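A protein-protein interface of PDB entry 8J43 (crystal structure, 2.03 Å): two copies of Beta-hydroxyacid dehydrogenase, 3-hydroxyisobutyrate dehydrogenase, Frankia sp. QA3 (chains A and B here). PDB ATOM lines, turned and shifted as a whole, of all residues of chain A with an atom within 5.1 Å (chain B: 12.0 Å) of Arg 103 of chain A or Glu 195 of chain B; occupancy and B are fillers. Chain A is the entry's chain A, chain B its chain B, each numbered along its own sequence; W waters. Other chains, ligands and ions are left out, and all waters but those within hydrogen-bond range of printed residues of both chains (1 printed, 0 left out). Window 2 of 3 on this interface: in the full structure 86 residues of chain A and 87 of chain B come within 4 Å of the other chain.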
ATOM      1  N   PRO A  99       7.090 -15.532  12.198  1.00  0.00           N
ATOM      2  CA  PRO A  99       8.540 -15.508  11.983  1.00  0.00           C
ATOM      3  C   PRO A  99       9.349 -15.603  13.297  1.00  0.00           C
ATOM      4  O   PRO A  99      10.411 -16.259  13.344  1.00  0.00           O
ATOM      5  CB  PRO A  99       8.764 -14.160  11.300  1.00  0.00           C
ATOM      6  CG  PRO A  99       7.477 -13.875  10.614  1.00  0.00           C
ATOM      7  CD  PRO A  99       6.419 -14.391  11.553  1.00  0.00           C
ATOM      8  N   GLU A 100       8.826 -14.978  14.346  1.00  0.00           N
ATOM      9  CA  GLU A 100       9.482 -14.915  15.640  1.00  0.00           C
ATOM     10  C   GLU A 100       9.538 -16.330  16.262  1.00  0.00           C
ATOM     11  O   GLU A 100      10.574 -16.758  16.785  1.00  0.00           O
ATOM     12  CB  GLU A 100       8.756 -13.893  16.550  1.00  0.00           C
ATOM     13  CG  GLU A 100       8.407 -12.554  15.854  1.00  0.00           C
ATOM     14  CD  GLU A 100       7.051 -12.564  15.110  1.00  0.00           C
ATOM     15  OE1 GLU A 100       6.153 -13.248  15.610  1.00  0.00           O
ATOM     16  OE2 GLU A 100       6.833 -11.920  14.051  1.00  0.00           O
ATOM     17  N   GLN A 101       8.440 -17.074  16.147  1.00  0.00           N
ATOM     18  CA  GLN A 101       8.402 -18.474  16.585  1.00  0.00           C
ATOM     19  C   GLN A 101       9.359 -19.378  15.824  1.00  0.00           C
ATOM     20  O   GLN A 101       9.942 -20.296  16.407  1.00  0.00           O
ATOM     21  CB  GLN A 101       6.997 -19.047  16.422  1.00  0.00           C
ATOM     22  CG  GLN A 101       6.002 -18.523  17.430  1.00  0.00           C
ATOM     23  CD  GLN A 101       4.645 -19.117  17.198  1.00  0.00           C
ATOM     24  OE1 GLN A 101       4.147 -19.163  16.074  1.00  0.00           O
ATOM     25  NE2 GLN A 101       4.047 -19.610  18.262  1.00  0.00           N
ATOM     26  N   ALA A 102       9.476 -19.135  14.521  1.00  0.00           N
ATOM     27  CA  ALA A 102      10.370 -19.913  13.665  1.00  0.00           C
ATOM     28  C   ALA A 102      11.828 -19.725  14.072  1.00  0.00           C
ATOM     29  O   ALA A 102      12.586 -20.689  14.088  1.00  0.00           O
ATOM     30  CB  ALA A 102      10.186 -19.537  12.196  1.00  0.00           C
ATOM     31  N   ARG A 103      12.218 -18.488  14.374  1.00  0.00           N
ATOM     32  CA  ARG A 103      13.610 -18.216  14.756  1.00  0.00           C
ATOM     33  C   ARG A 103      13.919 -18.786  16.131  1.00  0.00           C
ATOM     34  O   ARG A 103      14.997 -19.320  16.347  1.00  0.00           O
ATOM     35  CB  ARG A 103      13.935 -16.721  14.645  1.00  0.00           C
ATOM     36  CG  ARG A 103      13.956 -16.280  13.184  1.00  0.00           C
ATOM     37  CD  ARG A 103      14.367 -14.838  12.932  1.00  0.00           C
ATOM     38  NE  ARG A 103      13.335 -13.880  13.305  1.00  0.00           N
ATOM     39  CZ  ARG A 103      12.659 -13.072  12.477  1.00  0.00           C
ATOM     40  NH1 ARG A 103      11.763 -12.251  13.014  1.00  0.00           N
ATOM     41  NH2 ARG A 103      12.844 -13.077  11.150  1.00  0.00           N
ATOM     42  N   GLU A 104      12.959 -18.727  17.043  1.00  0.00           N
ATOM     43  CA  GLU A 104      13.137 -19.345  18.359  1.00  0.00           C
ATOM     44  C   GLU A 104      13.283 -20.860  18.258  1.00  0.00           C
ATOM     45  O   GLU A 104      14.109 -21.462  18.949  1.00  0.00           O
ATOM     46  CB  GLU A 104      11.962 -19.011  19.275  1.00  0.00           C
ATOM     47  CG  GLU A 104      11.972 -17.562  19.746  1.00  0.00           C
ATOM     48  CD  GLU A 104      10.787 -17.231  20.631  1.00  0.00           C
ATOM     49  OE1 GLU A 104      10.130 -18.180  21.138  1.00  0.00           O
ATOM     50  OE2 GLU A 104      10.525 -16.026  20.839  1.00  0.00           O
ATOM     51  N   ALA A 105      12.462 -21.474  17.410  1.00  0.00           N
ATOM     52  CA  ALA A 105      12.471 -22.932  17.260  1.00  0.00           C
ATOM     53  C   ALA A 105      13.801 -23.417  16.695  1.00  0.00           C
ATOM     54  O   ALA A 105      14.297 -24.453  17.099  1.00  0.00           O
ATOM     55  CB  ALA A 105      11.298 -23.406  16.398  1.00  0.00           C
ATOM     56  N   MET A 106      14.385 -22.656  15.776  1.00  0.00           N
ATOM     57  CA  MET A 106      15.688 -23.015  15.240  1.00  0.00           C
ATOM     58  C   MET A 106      16.763 -22.963  16.317  1.00  0.00           C
ATOM     59  O   MET A 106      17.603 -23.866  16.400  1.00  0.00           O
ATOM     60  CB  MET A 106      16.114 -22.094  14.107  1.00  0.00           C
ATOM     61  CG  MET A 106      17.472 -22.520  13.549  1.00  0.00           C
ATOM     62  SD  MET A 106      17.985 -21.631  12.085  1.00  0.00           S
ATOM     63  CE  MET A 106      16.893 -22.333  10.880  1.00  0.00           C
ATOM     64  N   ALA A 107      16.762 -21.898  17.113  1.00  0.00           N
ATOM     65  CA  ALA A 107      17.736 -21.764  18.197  1.00  0.00           C
ATOM     66  C   ALA A 107      17.589 -22.951  19.160  1.00  0.00           C
ATOM     67  O   ALA A 107      18.577 -23.604  19.499  1.00  0.00           O
ATOM     68  CB  ALA A 107      17.572 -20.436  18.925  1.00  0.00           C
ATOM     69  N   ASP A 163      17.532 -17.133   6.973  1.00  0.00           N
ATOM     70  CA  ASP A 163      16.643 -16.798   8.096  1.00  0.00           C
ATOM     71  C   ASP A 163      15.410 -17.738   8.126  1.00  0.00           C
ATOM     72  O   ASP A 163      14.638 -17.751   7.177  1.00  0.00           O
ATOM     73  CB  ASP A 163      16.207 -15.340   8.003  1.00  0.00           C
ATOM     74  CG  ASP A 163      15.185 -14.960   9.049  1.00  0.00           C
ATOM     75  OD1 ASP A 163      15.019 -15.686  10.041  1.00  0.00           O
ATOM     76  OD2 ASP A 163      14.536 -13.905   8.889  1.00  0.00           O
ATOM     77  N   PRO A 164      15.233 -18.531   9.210  1.00  0.00           N
ATOM     78  CA  PRO A 164      14.043 -19.407   9.273  1.00  0.00           C
ATOM     79  C   PRO A 164      12.715 -18.677   9.310  1.00  0.00           C
ATOM     80  O   PRO A 164      11.718 -19.234   8.858  1.00  0.00           O
ATOM     81  CB  PRO A 164      14.229 -20.190  10.576  1.00  0.00           C
ATOM     82  CG  PRO A 164      15.175 -19.366  11.387  1.00  0.00           C
ATOM     83  CD  PRO A 164      16.104 -18.724  10.385  1.00  0.00           C
ATOM     84  N   GLY A 165      12.698 -17.445   9.822  1.00  0.00           N
ATOM     85  CA  GLY A 165      11.473 -16.654   9.878  1.00  0.00           C
ATOM     86  C   GLY A 165      10.934 -16.255   8.505  1.00  0.00           C
ATOM     87  O   GLY A 165       9.773 -15.869   8.380  1.00  0.00           O
ATOM     88  N   LEU A 166      11.769 -16.352   7.471  1.00  0.00           N
ATOM     89  CA  LEU A 166      11.339 -15.949   6.130  1.00  0.00           C
ATOM     90  C   LEU A 166      10.168 -16.796   5.617  1.00  0.00           C
ATOM     91  O   LEU A 166       9.266 -16.268   4.971  1.00  0.00           O
ATOM     92  CB  LEU A 166      12.506 -16.004   5.137  1.00  0.00           C
ATOM     93  CG  LEU A 166      13.434 -14.765   5.115  1.00  0.00           C
ATOM     94  CD1 LEU A 166      14.733 -15.102   4.387  1.00  0.00           C
ATOM     95  CD2 LEU A 166      12.763 -13.558   4.476  1.00  0.00           C
ATOM     96  N   LEU A 169       7.128 -15.564   7.350  1.00  0.00           N
ATOM     97  CA  LEU A 169       6.848 -14.199   6.895  1.00  0.00           C
ATOM     98  C   LEU A 169       6.043 -14.203   5.581  1.00  0.00           C
ATOM     99  O   LEU A 169       4.998 -13.539   5.459  1.00  0.00           O
ATOM    100  CB  LEU A 169       8.174 -13.449   6.701  1.00  0.00           C
ATOM    101  CG  LEU A 169       8.122 -11.975   6.269  1.00  0.00           C
ATOM    102  CD1 LEU A 169       7.767 -11.093   7.445  1.00  0.00           C
ATOM    103  CD2 LEU A 169       9.450 -11.547   5.650  1.00  0.00           C
ATOM    104  N   LEU B 186      -1.762  -6.242  -0.862  1.00  0.00           N
ATOM    105  CA  LEU B 186      -1.096  -5.022  -0.354  1.00  0.00           C
ATOM    106  C   LEU B 186      -0.763  -5.131   1.136  1.00  0.00           C
ATOM    107  O   LEU B 186       0.318  -4.724   1.571  1.00  0.00           O
ATOM    108  CB  LEU B 186      -1.939  -3.769  -0.610  1.00  0.00           C
ATOM    109  CG  LEU B 186      -2.002  -3.330  -2.078  1.00  0.00           C
ATOM    110  CD1 LEU B 186      -3.067  -2.273  -2.254  1.00  0.00           C
ATOM    111  CD2 LEU B 186      -0.674  -2.826  -2.613  1.00  0.00           C
ATOM    112  N   HIS B 187      -1.691  -5.697   1.900  1.00  0.00           N
ATOM    113  CA  HIS B 187      -1.454  -5.914   3.338  1.00  0.00           C
ATOM    114  C   HIS B 187      -0.230  -6.824   3.581  1.00  0.00           C
ATOM    115  O   HIS B 187       0.688  -6.469   4.335  1.00  0.00           O
ATOM    116  CB  HIS B 187      -2.708  -6.492   3.982  1.00  0.00           C
ATOM    117  CG  HIS B 187      -2.590  -6.704   5.451  1.00  0.00           C
ATOM    118  ND1 HIS B 187      -2.026  -7.841   5.992  1.00  0.00           N
ATOM    119  CD2 HIS B 187      -2.985  -5.942   6.495  1.00  0.00           C
ATOM    120  CE1 HIS B 187      -2.082  -7.767   7.309  1.00  0.00           C
ATOM    121  NE2 HIS B 187      -2.673  -6.632   7.639  1.00  0.00           N
ATOM    122  N   GLY B 188      -0.201  -7.960   2.886  1.00  0.00           N
ATOM    123  CA  GLY B 188       0.932  -8.878   2.960  1.00  0.00           C
ATOM    124  C   GLY B 188       2.241  -8.284   2.464  1.00  0.00           C
ATOM    125  O   GLY B 188       3.291  -8.490   3.077  1.00  0.00           O
ATOM    126  N   THR B 189       2.172  -7.539   1.368  1.00  0.00           N
ATOM    127  CA  THR B 189       3.336  -6.842   0.835  1.00  0.00           C
ATOM    128  C   THR B 189       3.921  -5.827   1.841  1.00  0.00           C
ATOM    129  O   THR B 189       5.128  -5.754   2.016  1.00  0.00           O
ATOM    130  CB  THR B 189       2.996  -6.176  -0.513  1.00  0.00           C
ATOM    131  OG1 THR B 189       2.616  -7.188  -1.461  1.00  0.00           O
ATOM    132  CG2 THR B 189       4.162  -5.456  -1.064  1.00  0.00           C
ATOM    133  N   ALA B 190       3.069  -5.057   2.505  1.00  0.00           N
ATOM    134  CA  ALA B 190       3.507  -4.165   3.583  1.00  0.00           C
ATOM    135  C   ALA B 190       4.270  -4.959   4.655  1.00  0.00           C
ATOM    136  O   ALA B 190       5.361  -4.587   5.097  1.00  0.00           O
ATOM    137  CB  ALA B 190       2.308  -3.465   4.192  1.00  0.00           C
ATOM    138  N   LEU B 191       3.701  -6.093   5.027  1.00  0.00           N
ATOM    139  CA  LEU B 191       4.273  -6.941   6.050  1.00  0.00           C
ATOM    140  C   LEU B 191       5.685  -7.429   5.701  1.00  0.00           C
ATOM    141  O   LEU B 191       6.626  -7.193   6.448  1.00  0.00           O
ATOM    142  CB  LEU B 191       3.323  -8.116   6.253  1.00  0.00           C
ATOM    143  CG  LEU B 191       3.478  -8.959   7.490  1.00  0.00           C
ATOM    144  CD1 LEU B 191       2.108  -9.522   7.838  1.00  0.00           C
ATOM    145  CD2 LEU B 191       4.477 -10.074   7.261  1.00  0.00           C
ATOM    146  N   VAL B 192       5.849  -8.094   4.557  1.00  0.00           N
ATOM    147  CA  VAL B 192       7.176  -8.614   4.188  1.00  0.00           C
ATOM    148  C   VAL B 192       8.117  -7.457   3.890  1.00  0.00           C
ATOM    149  O   VAL B 192       9.303  -7.588   4.073  1.00  0.00           O
ATOM    150  CB  VAL B 192       7.151  -9.631   3.013  1.00  0.00           C
ATOM    151  CG1 VAL B 192       6.076 -10.693   3.250  1.00  0.00           C
ATOM    152  CG2 VAL B 192       6.965  -8.956   1.673  1.00  0.00           C
ATOM    153  N   GLY B 193       7.569  -6.331   3.439  1.00  0.00           N
ATOM    154  CA  GLY B 193       8.352  -5.111   3.156  1.00  0.00           C
ATOM    155  C   GLY B 193       9.034  -4.490   4.366  1.00  0.00           C
ATOM    156  O   GLY B 193      10.151  -3.998   4.266  1.00  0.00           O
ATOM    157  N   ALA B 194       8.368  -4.532   5.515  1.00  0.00           N
ATOM    158  CA  ALA B 194       8.991  -4.149   6.788  1.00  0.00           C
ATOM    159  C   ALA B 194      10.257  -4.957   7.089  1.00  0.00           C
ATOM    160  O   ALA B 194      11.119  -4.491   7.814  1.00  0.00           O
ATOM    161  CB  ALA B 194       7.993  -4.289   7.929  1.00  0.00           C
ATOM    162  N   GLU B 195      10.365  -6.162   6.529  1.00  0.00           N
ATOM    163  CA  GLU B 195      11.581  -6.971   6.637  1.00  0.00           C
ATOM    164  C   GLU B 195      12.532  -6.817   5.466  1.00  0.00           C
ATOM    165  O   GLU B 195      13.428  -7.621   5.327  1.00  0.00           O
ATOM    166  CB  GLU B 195      11.211  -8.449   6.760  1.00  0.00           C
ATOM    167  CG  GLU B 195      10.310  -8.729   7.941  1.00  0.00           C
ATOM    168  CD  GLU B 195      11.075  -8.887   9.225  1.00  0.00           C
ATOM    169  OE1 GLU B 195      11.748  -9.923   9.369  1.00  0.00           O
ATOM    170  OE2 GLU B 195      10.976  -7.998  10.092  1.00  0.00           O
ATOM    171  N   LYS B 196      12.339  -5.801   4.629  1.00  0.00           N
ATOM    172  CA  LYS B 196      13.214  -5.535   3.480  1.00  0.00           C
ATOM    173  C   LYS B 196      13.144  -6.558   2.350  1.00  0.00           C
ATOM    174  O   LYS B 196      14.052  -6.644   1.539  1.00  0.00           O
ATOM    175  CB  LYS B 196      14.669  -5.313   3.916  1.00  0.00           C
ATOM    176  CG  LYS B 196      14.821  -4.216   4.963  1.00  0.00           C
ATOM    177  CD  LYS B 196      16.098  -3.401   4.769  1.00  0.00           C
ATOM    178  CE  LYS B 196      16.410  -2.589   6.022  1.00  0.00           C
ATOM    179  NZ  LYS B 196      16.770  -3.492   7.160  1.00  0.00           N
ATOM    180  N   THR B 197      12.050  -7.316   2.291  1.00  0.00           N
ATOM    181  CA  THR B 197      11.687  -8.066   1.090  1.00  0.00           C
ATOM    182  C   THR B 197      10.884  -7.122   0.165  1.00  0.00           C
ATOM    183  O   THR B 197       9.795  -6.653   0.538  1.00  0.00           O
ATOM    184  CB  THR B 197      10.858  -9.325   1.444  1.00  0.00           C
ATOM    185  OG1 THR B 197      11.706 -10.284   2.089  1.00  0.00           O
ATOM    186  CG2 THR B 197      10.274  -9.968   0.206  1.00  0.00           C
ATOM    187  N   SER B 198      11.404  -6.860  -1.033  1.00  0.00           N
ATOM    188  CA  SER B 198      10.741  -5.941  -1.956  1.00  0.00           C
ATOM    189  C   SER B 198       9.444  -6.552  -2.478  1.00  0.00           C
ATOM    190  O   SER B 198       9.290  -7.775  -2.495  1.00  0.00           O
ATOM    191  CB  SER B 198      11.650  -5.619  -3.140  1.00  0.00           C
ATOM    192  OG  SER B 198      11.739  -6.744  -4.007  1.00  0.00           O
ATOM    193  N   ALA B 199       8.502  -5.694  -2.869  1.00  0.00           N
ATOM    194  CA  ALA B 199       7.246  -6.136  -3.499  1.00  0.00           C
ATOM    195  C   ALA B 199       7.541  -6.938  -4.765  1.00  0.00           C
ATOM    196  O   ALA B 199       6.850  -7.932  -5.065  1.00  0.00           O
ATOM    197  CB  ALA B 199       6.359  -4.948  -3.826  1.00  0.00           C
ATOM    198  N   THR B 200       8.583  -6.534  -5.482  1.00  0.00           N
ATOM    199  CA  THR B 200       8.961  -7.224  -6.720  1.00  0.00           C
ATOM    200  C   THR B 200       9.539  -8.617  -6.463  1.00  0.00           C
ATOM    201  O   THR B 200       9.433  -9.495  -7.319  1.00  0.00           O
ATOM    202  CB  THR B 200       9.933  -6.396  -7.573  1.00  0.00           C
ATOM    203  OG1 THR B 200      11.056  -5.998  -6.789  1.00  0.00           O
ATOM    204  CG2 THR B 200       9.247  -5.169  -8.122  1.00  0.00           C
ATOM    205  N   THR B 201      10.127  -8.823  -5.289  1.00  0.00           N
ATOM    206  CA  THR B 201      10.551 -10.158  -4.865  1.00  0.00           C
ATOM    207  C   THR B 201       9.378 -11.032  -4.386  1.00  0.00           C
ATOM    208  O   THR B 201       9.319 -12.216  -4.717  1.00  0.00           O
ATOM    209  CB  THR B 201      11.611 -10.056  -3.751  1.00  0.00           C
ATOM    210  OG1 THR B 201      12.687  -9.241  -4.212  1.00  0.00           O
ATOM    211  CG2 THR B 201      12.159 -11.433  -3.378  1.00  0.00           C
ATOM    212  N   PHE B 202       8.469 -10.454  -3.593  1.00  0.00           N
ATOM    213  CA  PHE B 202       7.353 -11.199  -3.006  1.00  0.00           C
ATOM    214  C   PHE B 202       6.292 -11.587  -4.043  1.00  0.00           C
ATOM    215  O   PHE B 202       5.704 -12.675  -3.984  1.00  0.00           O
ATOM    216  CB  PHE B 202       6.689 -10.388  -1.869  1.00  0.00           C
ATOM    217  CG  PHE B 202       5.442 -11.040  -1.285  1.00  0.00           C
ATOM    218  CD1 PHE B 202       5.511 -12.272  -0.649  1.00  0.00           C
ATOM    219  CD2 PHE B 202       4.203 -10.412  -1.344  1.00  0.00           C
ATOM    220  CE1 PHE B 202       4.374 -12.866  -0.094  1.00  0.00           C
ATOM    221  CE2 PHE B 202       3.066 -10.998  -0.777  1.00  0.00           C
ATOM    222  CZ  PHE B 202       3.153 -12.232  -0.161  1.00  0.00           C
ATOM    223  N   HIS B 245      -1.513 -15.686  13.627  1.00  0.00           N
ATOM    224  CA  HIS B 245      -0.105 -15.489  13.260  1.00  0.00           C
ATOM    225  C   HIS B 245       0.071 -14.298  12.303  1.00  0.00           C
ATOM    226  O   HIS B 245       1.017 -13.531  12.445  1.00  0.00           O
ATOM    227  CB  HIS B 245       0.502 -16.758  12.658  1.00  0.00           C
ATOM    228  CG  HIS B 245       0.438 -17.943  13.575  1.00  0.00           C
ATOM    229  ND1 HIS B 245       0.041 -19.195  13.154  1.00  0.00           N
ATOM    230  CD2 HIS B 245       0.673 -18.049  14.904  1.00  0.00           C
ATOM    231  CE1 HIS B 245       0.047 -20.021  14.185  1.00  0.00           C
ATOM    232  NE2 HIS B 245       0.437 -19.351  15.255  1.00  0.00           N
ATOM    233  N   LEU B 246      -0.841 -14.153  11.343  1.00  0.00           N
ATOM    234  CA  LEU B 246      -0.847 -12.995  10.465  1.00  0.00           C
ATOM    235  C   LEU B 246      -1.078 -11.704  11.261  1.00  0.00           C
ATOM    236  O   LEU B 246      -0.336 -10.723  11.108  1.00  0.00           O
ATOM    237  CB  LEU B 246      -1.933 -13.156   9.396  1.00  0.00           C
ATOM    238  CG  LEU B 246      -2.237 -11.932   8.548  1.00  0.00           C
ATOM    239  CD1 LEU B 246      -0.974 -11.512   7.834  1.00  0.00           C
ATOM    240  CD2 LEU B 246      -3.370 -12.184   7.563  1.00  0.00           C
ATOM    241  N   HIS B 248      -0.583 -11.021  14.492  1.00  0.00           N
ATOM    242  CA  HIS B 248       0.597 -10.799  15.333  1.00  0.00           C
ATOM    243  C   HIS B 248       1.797 -10.269  14.511  1.00  0.00           C
ATOM    244  O   HIS B 248       2.439  -9.279  14.873  1.00  0.00           O
ATOM    245  CB  HIS B 248       0.937 -12.121  16.062  1.00  0.00           C
ATOM    246  CG  HIS B 248       2.172 -12.069  16.915  1.00  0.00           C
ATOM    247  ND1 HIS B 248       2.164 -11.630  18.224  1.00  0.00           N
ATOM    248  CD2 HIS B 248       3.459 -12.403  16.641  1.00  0.00           C
ATOM    249  CE1 HIS B 248       3.390 -11.700  18.719  1.00  0.00           C
ATOM    250  NE2 HIS B 248       4.196 -12.154  17.775  1.00  0.00           N
ATOM    251  N   ALA B 249       2.094 -10.916  13.396  1.00  0.00           N
ATOM    252  CA  ALA B 249       3.198 -10.485  12.563  1.00  0.00           C
ATOM    253  C   ALA B 249       2.984  -9.065  12.023  1.00  0.00           C
ATOM    254  O   ALA B 249       3.923  -8.283  11.950  1.00  0.00           O
ATOM    255  CB  ALA B 249       3.405 -11.459  11.412  1.00  0.00           C
ATOM    256  N   ALA B 250       1.755  -8.750  11.634  1.00  0.00           N
ATOM    257  CA  ALA B 250       1.426  -7.457  11.029  1.00  0.00           C
ATOM    258  C   ALA B 250       1.458  -6.342  12.077  1.00  0.00           C
ATOM    259  O   ALA B 250       2.056  -5.291  11.857  1.00  0.00           O
ATOM    260  CB  ALA B 250       0.060  -7.524  10.377  1.00  0.00           C
ATOM    261  N   ALA B 251       0.835  -6.599  13.228  1.00  0.00           N
ATOM    262  CA  ALA B 251       0.783  -5.649  14.348  1.00  0.00           C
ATOM    263  C   ALA B 251       2.172  -5.179  14.771  1.00  0.00           C
ATOM    264  O   ALA B 251       2.405  -4.007  14.955  1.00  0.00           O
ATOM    265  CB  ALA B 251       0.067  -6.278  15.527  1.00  0.00           C
ATOM    266  N   SER B 252       3.093  -6.115  14.890  1.00  0.00           N
ATOM    267  CA  SER B 252       4.473  -5.816  15.261  1.00  0.00           C
ATOM    268  C   SER B 252       5.272  -5.038  14.197  1.00  0.00           C
ATOM    269  O   SER B 252       6.340  -4.521  14.488  1.00  0.00           O
ATOM    270  CB  SER B 252       5.191  -7.134  15.600  1.00  0.00           C
ATOM    271  OG  SER B 252       6.455  -7.221  14.956  1.00  0.00           O
ATOM    272  N   ARG B 253       4.778  -4.992  12.964  1.00  0.00           N
ATOM    273  CA  ARG B 253       5.485  -4.339  11.869  1.00  0.00           C
ATOM    274  C   ARG B 253       4.738  -3.100  11.356  1.00  0.00           C
ATOM    275  O   ARG B 253       5.030  -2.591  10.280  1.00  0.00           O
ATOM    276  CB  ARG B 253       5.708  -5.351  10.748  1.00  0.00           C
ATOM    277  CG  ARG B 253       6.628  -6.499  11.162  1.00  0.00           C
ATOM    278  CD  ARG B 253       6.640  -7.644  10.174  1.00  0.00           C
ATOM    279  NE  ARG B 253       7.726  -8.561  10.487  1.00  0.00           N
ATOM    280  CZ  ARG B 253       7.709  -9.477  11.454  1.00  0.00           C
ATOM    281  NH1 ARG B 253       6.649  -9.620  12.238  1.00  0.00           N
ATOM    282  NH2 ARG B 253       8.779 -10.257  11.649  1.00  0.00           N
ATOM    283  N   GLY B 254       3.790  -2.614  12.144  1.00  0.00           N
ATOM    284  CA  GLY B 254       3.137  -1.341  11.872  1.00  0.00           C
ATOM    285  C   GLY B 254       2.142  -1.403  10.736  1.00  0.00           C
ATOM    286  O   GLY B 254       1.872  -0.402  10.109  1.00  0.00           O
ATOM    287  N   VAL B 255       1.572  -2.571  10.478  1.00  0.00           N
ATOM    288  CA  VAL B 255       0.605  -2.707   9.408  1.00  0.00           C
ATOM    289  C   VAL B 255      -0.797  -2.712   9.979  1.00  0.00           C
ATOM    290  O   VAL B 255      -1.094  -3.476  10.874  1.00  0.00           O
ATOM    291  CB  VAL B 255       0.870  -3.976   8.570  1.00  0.00           C
ATOM    292  CG1 VAL B 255      -0.072  -4.050   7.379  1.00  0.00           C
ATOM    293  CG2 VAL B 255       2.324  -3.983   8.102  1.00  0.00           C
HETATM  294  O   HOH W   1       2.385 -21.485  15.810  1.00  0.00           O
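Water W1 lies within hydrogen-bond range of OE1 of Gln 101 of chain A and NE2 of His 245 of chain B.
Arg 103 of chain A touches just these residues of chain B: Glu 195 (3.8 Å) and Arg 253 (3.8 Å). Glu 195 of chain B touches just these residues of chain A: Arg 103 (3.8 Å) and Leu 169 (3.5 Å). Of the printed residues of chain B, Pro 99 of chain A touches Arg 253. Glu 100 of chain A touches just these residues of chain B: His 248 and Arg 253. No residue of chain B comes within 4 Å of Ala 105 of chain A. No residue of chain B comes within 4 Å of Met 106 of chain A. No residue of chain B comes within 4 Å of Asp 163 of chain A. No residue of chain B comes within 4 Å of Gly 165 of chain A. Of the printed residues of chain A, Leu 191 of chain B touches Leu 169 (3.4 Å). Of the printed residues of chain A, His 248 of chain B touches Glu 100. Of the printed residues of chain A, Arg 253 of chain B touches Pro 99, Glu 100, Arg 103 and Leu 169. Of the printed residues of chain A, His 245 of chain B touches Gln 101. Printed residues of chain A within 4 Å of Val 192 of chain B: Leu 169. His 187 of chain B touches none of the printed residues of chain A. The nearest printed residue of chain A that does not touch Val 192 of chain B is Leu 166 of chain A (6.6 Å).
Pro 99 of chain A touches Arg 253 of chain B (CB to NH2, 3.9 Å). Gln 101 of chain A touches His 245 of chain B. Arg 253 of chain B touches Arg 103 of chain A. Leu 191 of chain B touches Leu 169 of chain A. Leu 169 of chain A touches Val 192 of chain B (O to CG1, 3.8 Å). CD1 of Leu 169 of chain A touches CG of Glu 195 of chain B, 3.5 Å away. Leu 169 of chain A touches Arg 253 of chain B (CD1 to NE, 3.96 Å).
The guanidinium group (NH1) of Arg 253 of chain B lies within salt-bridge range of the side-chain carboxylate (OE2) of Glu 100 of chain A. OE1 of Glu 100 of chain A lies close to NE2 of His 248 of chain B (3.1 Å). The guanidinium group of Arg 103 of chain A lies within salt-bridge range of the side-chain carboxylate of Glu 195 of chain B, 3.8 Å away.
Hydrophobic or aromatic side chains of chain A that line the printed part of chain B: Pro 99 and Leu 169. Of the 27 printed residues of chain B, 6 touch a printed residue of chain A. Hydrophobic or aromatic side chains of chain B that line the printed part of chain A: Leu 191, Val 192, His 245 and His 248. Among the printed residues, 10 pairs touch across the chains. Among the printed residues, Asp or Glu carboxylates within 4 Å of a Lys or Arg side-chain nitrogen of the other chain: Glu 100 of chain A with Arg 253 of chain B (2.9 Å) and Arg 103 of chain A with Glu 195 of chain B (3.8 Å).
NH2 of Arg 103 of chain A is in salt-bridge range of OD2 of Asp 163 of chain A (2.9 Å). N of Thr 197 of chain B sits at hydrogen-bond distance from O of Val 192 of chain B. The guanidinium group (NH1) of Arg 253 of chain B sits at hydrogen-bond distance from the backbone carbonyl oxygen (O) of Ala 249 of chain B. OE2 of Glu 195 of chain B lies within salt-bridge range of NE of Arg 253 of chain B (3.3 Å).
No position is printed for both chains.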
